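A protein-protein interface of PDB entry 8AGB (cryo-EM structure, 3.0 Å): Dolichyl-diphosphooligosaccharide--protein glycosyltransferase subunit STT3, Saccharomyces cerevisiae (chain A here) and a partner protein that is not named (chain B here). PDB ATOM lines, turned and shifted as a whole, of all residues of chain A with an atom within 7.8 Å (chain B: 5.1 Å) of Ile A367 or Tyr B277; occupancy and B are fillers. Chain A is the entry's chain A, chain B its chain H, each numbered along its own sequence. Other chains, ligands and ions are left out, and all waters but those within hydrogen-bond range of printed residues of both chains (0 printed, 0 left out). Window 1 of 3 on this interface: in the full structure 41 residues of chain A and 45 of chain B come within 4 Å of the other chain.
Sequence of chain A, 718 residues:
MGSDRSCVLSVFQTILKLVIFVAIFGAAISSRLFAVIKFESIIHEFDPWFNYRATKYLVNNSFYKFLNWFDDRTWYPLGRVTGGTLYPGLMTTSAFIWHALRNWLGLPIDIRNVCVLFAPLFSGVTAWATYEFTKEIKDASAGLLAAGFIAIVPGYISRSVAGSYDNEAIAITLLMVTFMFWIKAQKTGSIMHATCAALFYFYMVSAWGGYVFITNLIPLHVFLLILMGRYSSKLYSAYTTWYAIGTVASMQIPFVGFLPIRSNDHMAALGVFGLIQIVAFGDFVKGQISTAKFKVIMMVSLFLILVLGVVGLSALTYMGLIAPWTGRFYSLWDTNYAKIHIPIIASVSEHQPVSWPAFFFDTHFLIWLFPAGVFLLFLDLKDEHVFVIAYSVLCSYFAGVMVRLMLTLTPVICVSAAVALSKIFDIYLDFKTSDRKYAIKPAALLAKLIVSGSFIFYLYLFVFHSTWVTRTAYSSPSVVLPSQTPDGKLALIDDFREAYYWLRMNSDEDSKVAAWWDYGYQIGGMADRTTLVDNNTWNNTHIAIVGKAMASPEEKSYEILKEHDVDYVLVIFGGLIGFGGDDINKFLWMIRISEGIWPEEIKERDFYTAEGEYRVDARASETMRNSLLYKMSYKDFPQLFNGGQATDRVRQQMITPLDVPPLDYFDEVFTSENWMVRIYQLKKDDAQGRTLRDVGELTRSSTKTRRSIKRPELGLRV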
ATOM      1  N   TRP A 356       1.135  -7.901  13.882  1.00  0.00           N
ATOM      2  CA  TRP A 356       0.788  -7.006  12.786  1.00  0.00           C
ATOM      3  C   TRP A 356      -0.705  -6.939  12.456  1.00  0.00           C
ATOM      4  O   TRP A 356      -1.189  -5.841  12.138  1.00  0.00           O
ATOM      5  CB  TRP A 356       1.591  -7.384  11.534  1.00  0.00           C
ATOM      6  CG  TRP A 356       1.094  -8.573  10.772  1.00  0.00           C
ATOM      7  CD1 TRP A 356       1.579  -9.842  10.838  1.00  0.00           C
ATOM      8  CD2 TRP A 356       0.042  -8.597   9.797  1.00  0.00           C
ATOM      9  NE1 TRP A 356       0.883 -10.660   9.985  1.00  0.00           N
ATOM     10  CE2 TRP A 356      -0.065  -9.919   9.334  1.00  0.00           C
ATOM     11  CE3 TRP A 356      -0.825  -7.631   9.282  1.00  0.00           C
ATOM     12  CZ2 TRP A 356      -1.003 -10.299   8.382  1.00  0.00           C
ATOM     13  CZ3 TRP A 356      -1.755  -8.011   8.338  1.00  0.00           C
ATOM     14  CH2 TRP A 356      -1.836  -9.332   7.897  1.00  0.00           C
ATOM     15  N   PRO A 357      -1.495  -8.019  12.577  1.00  0.00           N
ATOM     16  CA  PRO A 357      -2.899  -7.913  12.147  1.00  0.00           C
ATOM     17  C   PRO A 357      -3.675  -6.875  12.918  1.00  0.00           C
ATOM     18  O   PRO A 357      -4.595  -6.266  12.354  1.00  0.00           O
ATOM     19  CB  PRO A 357      -3.459  -9.321  12.391  1.00  0.00           C
ATOM     20  CG  PRO A 357      -2.290 -10.198  12.429  1.00  0.00           C
ATOM     21  CD  PRO A 357      -1.191  -9.393  13.023  1.00  0.00           C
ATOM     22  N   ALA A 358      -3.251  -6.554  14.140  1.00  0.00           N
ATOM     23  CA  ALA A 358      -4.029  -5.626  14.941  1.00  0.00           C
ATOM     24  C   ALA A 358      -3.955  -4.238  14.342  1.00  0.00           C
ATOM     25  O   ALA A 358      -4.955  -3.510  14.344  1.00  0.00           O
ATOM     26  CB  ALA A 358      -3.528  -5.620  16.385  1.00  0.00           C
ATOM     27  N   PHE A 359      -2.818  -3.895  13.730  1.00  0.00           N
ATOM     28  CA  PHE A 359      -2.711  -2.585  13.105  1.00  0.00           C
ATOM     29  C   PHE A 359      -3.723  -2.462  11.980  1.00  0.00           C
ATOM     30  O   PHE A 359      -4.301  -1.391  11.766  1.00  0.00           O
ATOM     31  CB  PHE A 359      -1.292  -2.349  12.590  1.00  0.00           C
ATOM     32  CG  PHE A 359      -0.295  -2.064  13.673  1.00  0.00           C
ATOM     33  CD1 PHE A 359      -0.207  -0.805  14.234  1.00  0.00           C
ATOM     34  CD2 PHE A 359       0.553  -3.055  14.132  1.00  0.00           C
ATOM     35  CE1 PHE A 359       0.708  -0.537  15.228  1.00  0.00           C
ATOM     36  CE2 PHE A 359       1.469  -2.794  15.126  1.00  0.00           C
ATOM     37  CZ  PHE A 359       1.547  -1.534  15.674  1.00  0.00           C
ATOM     38  N   PHE A 360      -3.945  -3.551  11.241  1.00  0.00           N
ATOM     39  CA  PHE A 360      -4.973  -3.513  10.211  1.00  0.00           C
ATOM     40  C   PHE A 360      -6.360  -3.572  10.834  1.00  0.00           C
ATOM     41  O   PHE A 360      -7.301  -2.954  10.326  1.00  0.00           O
ATOM     42  CB  PHE A 360      -4.779  -4.650   9.213  1.00  0.00           C
ATOM     43  CG  PHE A 360      -5.783  -4.645   8.099  1.00  0.00           C
ATOM     44  CD1 PHE A 360      -5.640  -3.786   7.027  1.00  0.00           C
ATOM     45  CD2 PHE A 360      -6.873  -5.493   8.124  1.00  0.00           C
ATOM     46  CE1 PHE A 360      -6.561  -3.775   6.005  1.00  0.00           C
ATOM     47  CE2 PHE A 360      -7.795  -5.486   7.102  1.00  0.00           C
ATOM     48  CZ  PHE A 360      -7.639  -4.626   6.043  1.00  0.00           C
ATOM     49  N   PHE A 361      -6.507  -4.332  11.921  1.00  0.00           N
ATOM     50  CA  PHE A 361      -7.799  -4.429  12.591  1.00  0.00           C
ATOM     51  C   PHE A 361      -8.295  -3.060  13.035  1.00  0.00           C
ATOM     52  O   PHE A 361      -9.453  -2.699  12.802  1.00  0.00           O
ATOM     53  CB  PHE A 361      -7.698  -5.381  13.781  1.00  0.00           C
ATOM     54  CG  PHE A 361      -9.013  -5.961  14.204  1.00  0.00           C
ATOM     55  CD1 PHE A 361      -9.758  -6.728  13.330  1.00  0.00           C
ATOM     56  CD2 PHE A 361      -9.502  -5.743  15.477  1.00  0.00           C
ATOM     57  CE1 PHE A 361     -10.965  -7.264  13.716  1.00  0.00           C
ATOM     58  CE2 PHE A 361     -10.710  -6.276  15.869  1.00  0.00           C
ATOM     59  CZ  PHE A 361     -11.443  -7.037  14.987  1.00  0.00           C
ATOM     60  N   ASP A 362      -7.424  -2.279  13.670  1.00  0.00           N
ATOM     61  CA  ASP A 362      -7.839  -1.008  14.247  1.00  0.00           C
ATOM     62  C   ASP A 362      -7.949   0.100  13.207  1.00  0.00           C
ATOM     63  O   ASP A 362      -8.800   0.982  13.347  1.00  0.00           O
ATOM     64  CB  ASP A 362      -6.868  -0.596  15.351  1.00  0.00           C
ATOM     65  CG  ASP A 362      -7.075  -1.384  16.629  1.00  0.00           C
ATOM     66  OD1 ASP A 362      -8.235  -1.511  17.071  1.00  0.00           O
ATOM     67  OD2 ASP A 362      -6.077  -1.880  17.191  1.00  0.00           O
ATOM     68  N   THR A 363      -7.103   0.096  12.180  1.00  0.00           N
ATOM     69  CA  THR A 363      -7.211   1.054  11.084  1.00  0.00           C
ATOM     70  C   THR A 363      -7.231   0.312   9.757  1.00  0.00           C
ATOM     71  O   THR A 363      -6.281  -0.404   9.429  1.00  0.00           O
ATOM     72  CB  THR A 363      -6.052   2.050  11.113  1.00  0.00           C
ATOM     73  OG1 THR A 363      -4.811   1.336  11.088  1.00  0.00           O
ATOM     74  CG2 THR A 363      -6.112   2.898  12.370  1.00  0.00           C
ATOM     75  N   HIS A 364      -8.307   0.487   9.000  1.00  0.00           N
ATOM     76  CA  HIS A 364      -8.469  -0.131   7.691  1.00  0.00           C
ATOM     77  C   HIS A 364      -8.167   0.880   6.598  1.00  0.00           C
ATOM     78  O   HIS A 364      -8.678   2.003   6.637  1.00  0.00           O
ATOM     79  CB  HIS A 364      -9.892  -0.658   7.518  1.00  0.00           C
ATOM     80  CG  HIS A 364     -10.212  -1.085   6.122  1.00  0.00           C
ATOM     81  ND1 HIS A 364     -10.894  -0.279   5.239  1.00  0.00           N
ATOM     82  CD2 HIS A 364      -9.964  -2.239   5.462  1.00  0.00           C
ATOM     83  CE1 HIS A 364     -11.040  -0.912   4.090  1.00  0.00           C
ATOM     84  NE2 HIS A 364     -10.487  -2.105   4.200  1.00  0.00           N
ATOM     85  N   PHE A 365      -7.301   0.499   5.655  1.00  0.00           N
ATOM     86  CA  PHE A 365      -7.029   1.301   4.464  1.00  0.00           C
ATOM     87  C   PHE A 365      -6.221   2.543   4.827  1.00  0.00           C
ATOM     88  O   PHE A 365      -5.718   3.251   3.951  1.00  0.00           O
ATOM     89  CB  PHE A 365      -8.348   1.621   3.738  1.00  0.00           C
ATOM     90  CG  PHE A 365      -8.495   3.047   3.283  1.00  0.00           C
ATOM     91  CD1 PHE A 365      -9.071   3.996   4.107  1.00  0.00           C
ATOM     92  CD2 PHE A 365      -8.091   3.429   2.018  1.00  0.00           C
ATOM     93  CE1 PHE A 365      -9.225   5.298   3.684  1.00  0.00           C
ATOM     94  CE2 PHE A 365      -8.240   4.734   1.595  1.00  0.00           C
ATOM     95  CZ  PHE A 365      -8.807   5.666   2.430  1.00  0.00           C
ATOM     96  N   LEU A 366      -6.058   2.783   6.126  1.00  0.00           N
ATOM     97  CA  LEU A 366      -5.389   3.965   6.640  1.00  0.00           C
ATOM     98  C   LEU A 366      -4.013   3.650   7.196  1.00  0.00           C
ATOM     99  O   LEU A 366      -3.287   4.575   7.571  1.00  0.00           O
ATOM    100  CB  LEU A 366      -6.229   4.610   7.751  1.00  0.00           C
ATOM    101  CG  LEU A 366      -7.536   5.305   7.387  1.00  0.00           C
ATOM    102  CD1 LEU A 366      -8.156   5.911   8.632  1.00  0.00           C
ATOM    103  CD2 LEU A 366      -7.311   6.358   6.331  1.00  0.00           C
ATOM    104  N   ILE A 367      -3.642   2.373   7.261  1.00  0.00           N
ATOM    105  CA  ILE A 367      -2.312   1.994   7.716  1.00  0.00           C
ATOM    106  C   ILE A 367      -1.259   2.273   6.648  1.00  0.00           C
ATOM    107  O   ILE A 367      -0.181   2.786   6.957  1.00  0.00           O
ATOM    108  CB  ILE A 367      -2.308   0.525   8.190  1.00  0.00           C
ATOM    109  CG1 ILE A 367      -1.071   0.243   9.043  1.00  0.00           C
ATOM    110  CG2 ILE A 367      -2.456  -0.462   7.035  1.00  0.00           C
ATOM    111  CD1 ILE A 367      -1.100   0.926  10.388  1.00  0.00           C
ATOM    112  N   TRP A 368      -1.525   1.919   5.385  1.00  0.00           N
ATOM    113  CA  TRP A 368      -0.549   2.202   4.332  1.00  0.00           C
ATOM    114  C   TRP A 368      -0.452   3.696   4.031  1.00  0.00           C
ATOM    115  O   TRP A 368       0.646   4.216   3.803  1.00  0.00           O
ATOM    116  CB  TRP A 368      -0.845   1.393   3.066  1.00  0.00           C
ATOM    117  CG  TRP A 368      -2.276   1.185   2.696  1.00  0.00           C
ATOM    118  CD1 TRP A 368      -3.129   0.265   3.222  1.00  0.00           C
ATOM    119  CD2 TRP A 368      -2.992   1.838   1.642  1.00  0.00           C
ATOM    120  NE1 TRP A 368      -4.348   0.339   2.598  1.00  0.00           N
ATOM    121  CE2 TRP A 368      -4.289   1.297   1.622  1.00  0.00           C
ATOM    122  CE3 TRP A 368      -2.670   2.848   0.731  1.00  0.00           C
ATOM    123  CZ2 TRP A 368      -5.263   1.727   0.726  1.00  0.00           C
ATOM    124  CZ3 TRP A 368      -3.639   3.272  -0.157  1.00  0.00           C
ATOM    125  CH2 TRP A 368      -4.918   2.714  -0.152  1.00  0.00           C
ATOM    126  N   LEU A 369      -1.588   4.394   3.998  1.00  0.00           N
ATOM    127  CA  LEU A 369      -1.595   5.829   3.715  1.00  0.00           C
ATOM    128  C   LEU A 369      -0.824   6.640   4.751  1.00  0.00           C
ATOM    129  O   LEU A 369      -0.336   7.730   4.439  1.00  0.00           O
ATOM    130  CB  LEU A 369      -3.033   6.341   3.645  1.00  0.00           C
ATOM    131  CG  LEU A 369      -3.829   6.127   2.364  1.00  0.00           C
ATOM    132  CD1 LEU A 369      -5.188   6.781   2.489  1.00  0.00           C
ATOM    133  CD2 LEU A 369      -3.072   6.702   1.184  1.00  0.00           C
ATOM    134  N   PHE A 370      -0.713   6.140   5.978  1.00  0.00           N
ATOM    135  CA  PHE A 370       0.050   6.846   7.006  1.00  0.00           C
ATOM    136  C   PHE A 370       1.525   7.036   6.645  1.00  0.00           C
ATOM    137  O   PHE A 370       2.001   8.187   6.702  1.00  0.00           O
ATOM    138  CB  PHE A 370      -0.191   6.130   8.345  1.00  0.00           C
ATOM    139  CG  PHE A 370       0.786   6.466   9.427  1.00  0.00           C
ATOM    140  CD1 PHE A 370       0.946   7.767   9.858  1.00  0.00           C
ATOM    141  CD2 PHE A 370       1.490   5.466  10.071  1.00  0.00           C
ATOM    142  CE1 PHE A 370       1.825   8.072  10.871  1.00  0.00           C
ATOM    143  CE2 PHE A 370       2.367   5.765  11.088  1.00  0.00           C
ATOM    144  CZ  PHE A 370       2.536   7.070  11.487  1.00  0.00           C
ATOM    145  N   PRO A 371       2.299   6.003   6.269  1.00  0.00           N
ATOM    146  CA  PRO A 371       3.678   6.275   5.832  1.00  0.00           C
ATOM    147  C   PRO A 371       3.741   7.194   4.628  1.00  0.00           C
ATOM    148  O   PRO A 371       4.635   8.047   4.537  1.00  0.00           O
ATOM    149  CB  PRO A 371       4.190   4.874   5.499  1.00  0.00           C
ATOM    150  CG  PRO A 371       3.590   4.065   6.554  1.00  0.00           C
ATOM    151  CD  PRO A 371       2.158   4.574   6.596  1.00  0.00           C
ATOM    152  N   ALA A 372       2.805   7.035   3.692  1.00  0.00           N
ATOM    153  CA  ALA A 372       2.827   7.839   2.480  1.00  0.00           C
ATOM    154  C   ALA A 372       2.645   9.306   2.828  1.00  0.00           C
ATOM    155  O   ALA A 372       3.264  10.186   2.219  1.00  0.00           O
ATOM    156  CB  ALA A 372       1.742   7.368   1.519  1.00  0.00           C
ATOM    157  N   GLY A 373       1.804   9.585   3.816  1.00  0.00           N
ATOM    158  CA  GLY A 373       1.516  10.950   4.173  1.00  0.00           C
ATOM    159  C   GLY A 373       2.689  11.524   4.936  1.00  0.00           C
ATOM    160  O   GLY A 373       3.013  12.696   4.753  1.00  0.00           O
ATOM    161  N   MET A 406      -1.462   2.365  21.253  1.00  0.00           N
ATOM    162  CA  MET A 406      -2.088   2.541  19.943  1.00  0.00           C
ATOM    163  C   MET A 406      -3.096   3.685  19.959  1.00  0.00           C
ATOM    164  O   MET A 406      -3.262   4.399  18.958  1.00  0.00           O
ATOM    165  CB  MET A 406      -2.764   1.243  19.506  1.00  0.00           C
ATOM    166  CG  MET A 406      -3.011   1.151  18.013  1.00  0.00           C
ATOM    167  SD  MET A 406      -3.126  -0.553  17.448  1.00  0.00           S
ATOM    168  CE  MET A 406      -1.753  -1.287  18.330  1.00  0.00           C
ATOM    169  N   LEU A 409      -1.583   6.793  19.231  1.00  0.00           N
ATOM    170  CA  LEU A 409      -1.067   6.767  17.871  1.00  0.00           C
ATOM    171  C   LEU A 409      -2.154   6.979  16.831  1.00  0.00           C
ATOM    172  O   LEU A 409      -1.845   7.355  15.697  1.00  0.00           O
ATOM    173  CB  LEU A 409      -0.361   5.432  17.598  1.00  0.00           C
ATOM    174  CG  LEU A 409      -0.035   5.045  16.150  1.00  0.00           C
ATOM    175  CD1 LEU A 409       1.018   5.973  15.565  1.00  0.00           C
ATOM    176  CD2 LEU A 409       0.385   3.595  16.021  1.00  0.00           C
ATOM    177  N   ILE A 413      -2.180   8.916  12.924  1.00  0.00           N
ATOM    178  CA  ILE A 413      -2.503   8.090  11.765  1.00  0.00           C
ATOM    179  C   ILE A 413      -3.559   8.815  10.945  1.00  0.00           C
ATOM    180  O   ILE A 413      -3.390   9.054   9.745  1.00  0.00           O
ATOM    181  CB  ILE A 413      -2.981   6.694  12.197  1.00  0.00           C
ATOM    182  CG1 ILE A 413      -1.860   5.946  12.917  1.00  0.00           C
ATOM    183  CG2 ILE A 413      -3.477   5.912  10.994  1.00  0.00           C
ATOM    184  CD1 ILE A 413      -2.027   4.446  12.927  1.00  0.00           C
ATOM    185  N   SER A 416      -2.270  12.237   9.229  1.00  0.00           N
ATOM    186  CA  SER A 416      -1.410  11.973   8.077  1.00  0.00           C
ATOM    187  C   SER A 416      -2.197  11.378   6.915  1.00  0.00           C
ATOM    188  O   SER A 416      -2.010  11.774   5.757  1.00  0.00           O
ATOM    189  CB  SER A 416      -0.268  11.049   8.479  1.00  0.00           C
ATOM    190  OG  SER A 416      -0.555   9.727   8.084  1.00  0.00           O
ATOM    191  N   ALA A 417      -2.997  10.345   7.193  1.00  0.00           N
ATOM    192  CA  ALA A 417      -3.864   9.748   6.185  1.00  0.00           C
ATOM    193  C   ALA A 417      -4.639  10.828   5.448  1.00  0.00           C
ATOM    194  O   ALA A 417      -4.662  10.865   4.212  1.00  0.00           O
ATOM    195  CB  ALA A 417      -4.811   8.750   6.843  1.00  0.00           C
ATOM    196  N   ILE B 229       7.334   1.935   8.548  1.00  0.00           N
ATOM    197  CA  ILE B 229       6.776   0.733   7.932  1.00  0.00           C
ATOM    198  C   ILE B 229       7.267  -0.512   8.656  1.00  0.00           C
ATOM    199  O   ILE B 229       6.520  -1.483   8.828  1.00  0.00           O
ATOM    200  CB  ILE B 229       7.125   0.699   6.433  1.00  0.00           C
ATOM    201  CG1 ILE B 229       6.359   1.791   5.692  1.00  0.00           C
ATOM    202  CG2 ILE B 229       6.805  -0.653   5.835  1.00  0.00           C
ATOM    203  CD1 ILE B 229       6.679   1.863   4.224  1.00  0.00           C
ATOM    204  N   ILE B 232       5.245  -0.651  12.099  1.00  0.00           N
ATOM    205  CA  ILE B 232       3.840  -1.055  12.055  1.00  0.00           C
ATOM    206  C   ILE B 232       3.664  -2.472  11.539  1.00  0.00           C
ATOM    207  O   ILE B 232       2.553  -3.009  11.608  1.00  0.00           O
ATOM    208  CB  ILE B 232       2.984  -0.109  11.191  1.00  0.00           C
ATOM    209  CG1 ILE B 232       3.217  -0.379   9.704  1.00  0.00           C
ATOM    210  CG2 ILE B 232       3.258   1.339  11.549  1.00  0.00           C
ATOM    211  CD1 ILE B 232       2.639   0.679   8.794  1.00  0.00           C
ATOM    212  N   SER B 233       4.723  -3.090  11.021  1.00  0.00           N
ATOM    213  CA  SER B 233       4.676  -4.477  10.586  1.00  0.00           C
ATOM    214  C   SER B 233       5.056  -5.448  11.694  1.00  0.00           C
ATOM    215  O   SER B 233       5.463  -6.577  11.401  1.00  0.00           O
ATOM    216  CB  SER B 233       5.586  -4.682   9.375  1.00  0.00           C
ATOM    217  OG  SER B 233       5.420  -3.638   8.434  1.00  0.00           O
ATOM    218  N   MET B 273       4.917  -8.401   4.947  1.00  0.00           N
ATOM    219  CA  MET B 273       4.046  -7.239   5.116  1.00  0.00           C
ATOM    220  C   MET B 273       4.760  -5.940   4.776  1.00  0.00           C
ATOM    221  O   MET B 273       4.195  -5.083   4.086  1.00  0.00           O
ATOM    222  CB  MET B 273       3.494  -7.191   6.539  1.00  0.00           C
ATOM    223  CG  MET B 273       2.591  -8.359   6.894  1.00  0.00           C
ATOM    224  SD  MET B 273       1.448  -8.821   5.578  1.00  0.00           S
ATOM    225  CE  MET B 273       0.552  -7.290   5.331  1.00  0.00           C
ATOM    226  N   VAL B 274       6.010  -5.789   5.225  1.00  0.00           N
ATOM    227  CA  VAL B 274       6.792  -4.602   4.877  1.00  0.00           C
ATOM    228  C   VAL B 274       6.713  -4.354   3.379  1.00  0.00           C
ATOM    229  O   VAL B 274       6.202  -3.319   2.931  1.00  0.00           O
ATOM    230  CB  VAL B 274       8.248  -4.742   5.348  1.00  0.00           C
ATOM    231  CG1 VAL B 274       9.110  -3.701   4.675  1.00  0.00           C
ATOM    232  CG2 VAL B 274       8.328  -4.552   6.843  1.00  0.00           C
ATOM    233  N   LEU B 275       7.175  -5.329   2.588  1.00  0.00           N
ATOM    234  CA  LEU B 275       7.060  -5.253   1.138  1.00  0.00           C
ATOM    235  C   LEU B 275       5.685  -4.747   0.737  1.00  0.00           C
ATOM    236  O   LEU B 275       5.562  -3.705   0.082  1.00  0.00           O
ATOM    237  CB  LEU B 275       7.335  -6.622   0.509  1.00  0.00           C
ATOM    238  CG  LEU B 275       8.667  -7.288   0.842  1.00  0.00           C
ATOM    239  CD1 LEU B 275       8.616  -8.763   0.495  1.00  0.00           C
ATOM    240  CD2 LEU B 275       9.800  -6.601   0.102  1.00  0.00           C
ATOM    241  N   ILE B 276       4.639  -5.450   1.184  1.00  0.00           N
ATOM    242  CA  ILE B 276       3.270  -5.045   0.870  1.00  0.00           C
ATOM    243  C   ILE B 276       3.081  -3.573   1.199  1.00  0.00           C
ATOM    244  O   ILE B 276       2.847  -2.742   0.312  1.00  0.00           O
ATOM    245  CB  ILE B 276       2.258  -5.921   1.627  1.00  0.00           C
ATOM    246  CG1 ILE B 276       2.530  -7.403   1.373  1.00  0.00           C
ATOM    247  CG2 ILE B 276       0.842  -5.559   1.222  1.00  0.00           C
ATOM    248  CD1 ILE B 276       2.560  -7.775  -0.083  1.00  0.00           C
ATOM    249  N   TYR B 277       3.250  -3.223   2.477  1.00  0.00           N
ATOM    250  CA  TYR B 277       3.156  -1.824   2.870  1.00  0.00           C
ATOM    251  C   TYR B 277       4.125  -0.981   2.057  1.00  0.00           C
ATOM    252  O   TYR B 277       3.737   0.031   1.458  1.00  0.00           O
ATOM    253  CB  TYR B 277       3.440  -1.674   4.363  1.00  0.00           C
ATOM    254  CG  TYR B 277       2.359  -2.215   5.265  1.00  0.00           C
ATOM    255  CD1 TYR B 277       1.028  -2.188   4.882  1.00  0.00           C
ATOM    256  CD2 TYR B 277       2.673  -2.749   6.506  1.00  0.00           C
ATOM    257  CE1 TYR B 277       0.041  -2.683   5.709  1.00  0.00           C
ATOM    258  CE2 TYR B 277       1.695  -3.244   7.338  1.00  0.00           C
ATOM    259  CZ  TYR B 277       0.382  -3.208   6.937  1.00  0.00           C
ATOM    260  OH  TYR B 277      -0.593  -3.704   7.769  1.00  0.00           O
ATOM    261  N   GLY B 278       5.385  -1.419   1.987  1.00  0.00           N
ATOM    262  CA  GLY B 278       6.392  -0.657   1.278  1.00  0.00           C
ATOM    263  C   GLY B 278       5.995  -0.366  -0.148  1.00  0.00           C
ATOM    264  O   GLY B 278       6.398   0.652  -0.713  1.00  0.00           O
ATOM    265  N   THR B 279       5.202  -1.250  -0.752  1.00  0.00           N
ATOM    266  CA  THR B 279       4.746  -0.988  -2.108  1.00  0.00           C
ATOM    267  C   THR B 279       3.582  -0.009  -2.101  1.00  0.00           C
ATOM    268  O   THR B 279       3.610   1.002  -2.812  1.00  0.00           O
ATOM    269  CB  THR B 279       4.356  -2.296  -2.792  1.00  0.00           C
ATOM    270  OG1 THR B 279       5.507  -3.142  -2.887  1.00  0.00           O
ATOM    271  CG2 THR B 279       3.833  -2.023  -4.184  1.00  0.00           C
ATOM    272  N   LEU B 280       2.581  -0.267  -1.254  1.00  0.00           N
ATOM    273  CA  LEU B 280       1.340   0.497  -1.301  1.00  0.00           C
ATOM    274  C   LEU B 280       1.608   1.988  -1.171  1.00  0.00           C
ATOM    275  O   LEU B 280       1.375   2.758  -2.110  1.00  0.00           O
ATOM    276  CB  LEU B 280       0.389   0.018  -0.206  1.00  0.00           C
ATOM    277  CG  LEU B 280      -0.441  -1.212  -0.562  1.00  0.00           C
ATOM    278  CD1 LEU B 280      -1.034  -1.833   0.683  1.00  0.00           C
ATOM    279  CD2 LEU B 280      -1.531  -0.826  -1.539  1.00  0.00           C
ATOM    280  N   ALA B 281       2.132   2.407  -0.015  1.00  0.00           N
ATOM    281  CA  ALA B 281       2.538   3.795   0.175  1.00  0.00           C
ATOM    282  C   ALA B 281       3.339   4.303  -1.014  1.00  0.00           C
ATOM    283  O   ALA B 281       3.047   5.373  -1.561  1.00  0.00           O
ATOM    284  CB  ALA B 281       3.348   3.930   1.464  1.00  0.00           C
ATOM    285  N   ALA B 282       4.338   3.528  -1.443  1.00  0.00           N
ATOM    286  CA  ALA B 282       5.169   3.935  -2.572  1.00  0.00           C
ATOM    287  C   ALA B 282       4.316   4.366  -3.754  1.00  0.00           C
ATOM    288  O   ALA B 282       4.469   5.479  -4.272  1.00  0.00           O
ATOM    289  CB  ALA B 282       6.106   2.799  -2.976  1.00  0.00           C
ATOM    290  N   LEU B 327      -3.246  -7.592   0.493  1.00  0.00           N
ATOM    291  CA  LEU B 327      -3.253  -7.350   1.933  1.00  0.00           C
ATOM    292  C   LEU B 327      -4.485  -7.971   2.583  1.00  0.00           C
ATOM    293  O   LEU B 327      -4.387  -8.635   3.623  1.00  0.00           O
ATOM    294  CB  LEU B 327      -3.190  -5.846   2.207  1.00  0.00           C
ATOM    295  CG  LEU B 327      -3.571  -5.263   3.574  1.00  0.00           C
ATOM    296  CD1 LEU B 327      -2.953  -6.033   4.734  1.00  0.00           C
ATOM    297  CD2 LEU B 327      -3.179  -3.798   3.644  1.00  0.00           C
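The backbone carbonyl oxygen of Phe A365 sits close to the indole nitrogen of Trp A368, at 3.5 Å. The backbone carbonyl oxygen of Ile B229 is in hydrogen-bond range of the side-chain hydroxyl of Ser B233 (2.5 Å). The backbone carbonyl oxygen (O) of Phe A359 sits at hydrogen-bond distance from the side-chain hydroxyl (OG1) of Thr A363 (2.9 Å).
Ser B233 touches Trp A356 (O to CB, 3.96 Å). CE of Met B273 touches CZ3 of Trp A356 (3.9 Å). Ile B232 touches Phe A359. Ile A367 touches Ile B232 (CG1 to CD1, 3.7 Å). Ile A367 touches Tyr B277 (CG2 to CE1, 3.6 Å). Trp A368 touches Leu B280. Ala B281 touches Trp A368. CG1 of Ile B229 touches CG of Pro A371 (3.7 Å). Ala B281 touches Ala A372.
Printed residues of chain B within 4 Å of Trp A356: Ser B233 (3.96 Å) and Met B273 (3.9 Å). Printed residues of chain B within 4 Å of Phe A359: Ile B232 (3.2 Å). Of chain B, only Ile B232 and Tyr B277 come within 4 Å of Ile A367. Printed residues of chain B within 4 Å of Trp A368: Leu B280 (3.8 Å) and Ala B281 (3.6 Å). Of the printed residues of chain A, Ser B233 touches Trp A356. Tyr B277 touches just one residue of chain A: Ile A367 (3.6 Å). No residue of chain A comes within 4 Å of Gly B278. Of the printed residues of chain A, Ala B281 touches Trp A368 and Ala A372. The nearest residue of chain B that does not touch Ile A367 is Leu B327 (4.8 Å).
Printed residues of chain B that touch a printed residue of chain A: Ile B229, Ile B232, Ser B233, Met B273, Tyr B277, Leu B280 and Ala B281. Printed residues of chain A that touch a printed residue of chain B: Trp A356, Phe A359, Ile A367, Trp A368, Pro A371 and Ala A372. Hydrophobic or aromatic side chains of chain A within 4 Å of the printed part of chain B: Trp A356, Phe A359, Ile A367, Trp A368, Pro A371 and Ala A372.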
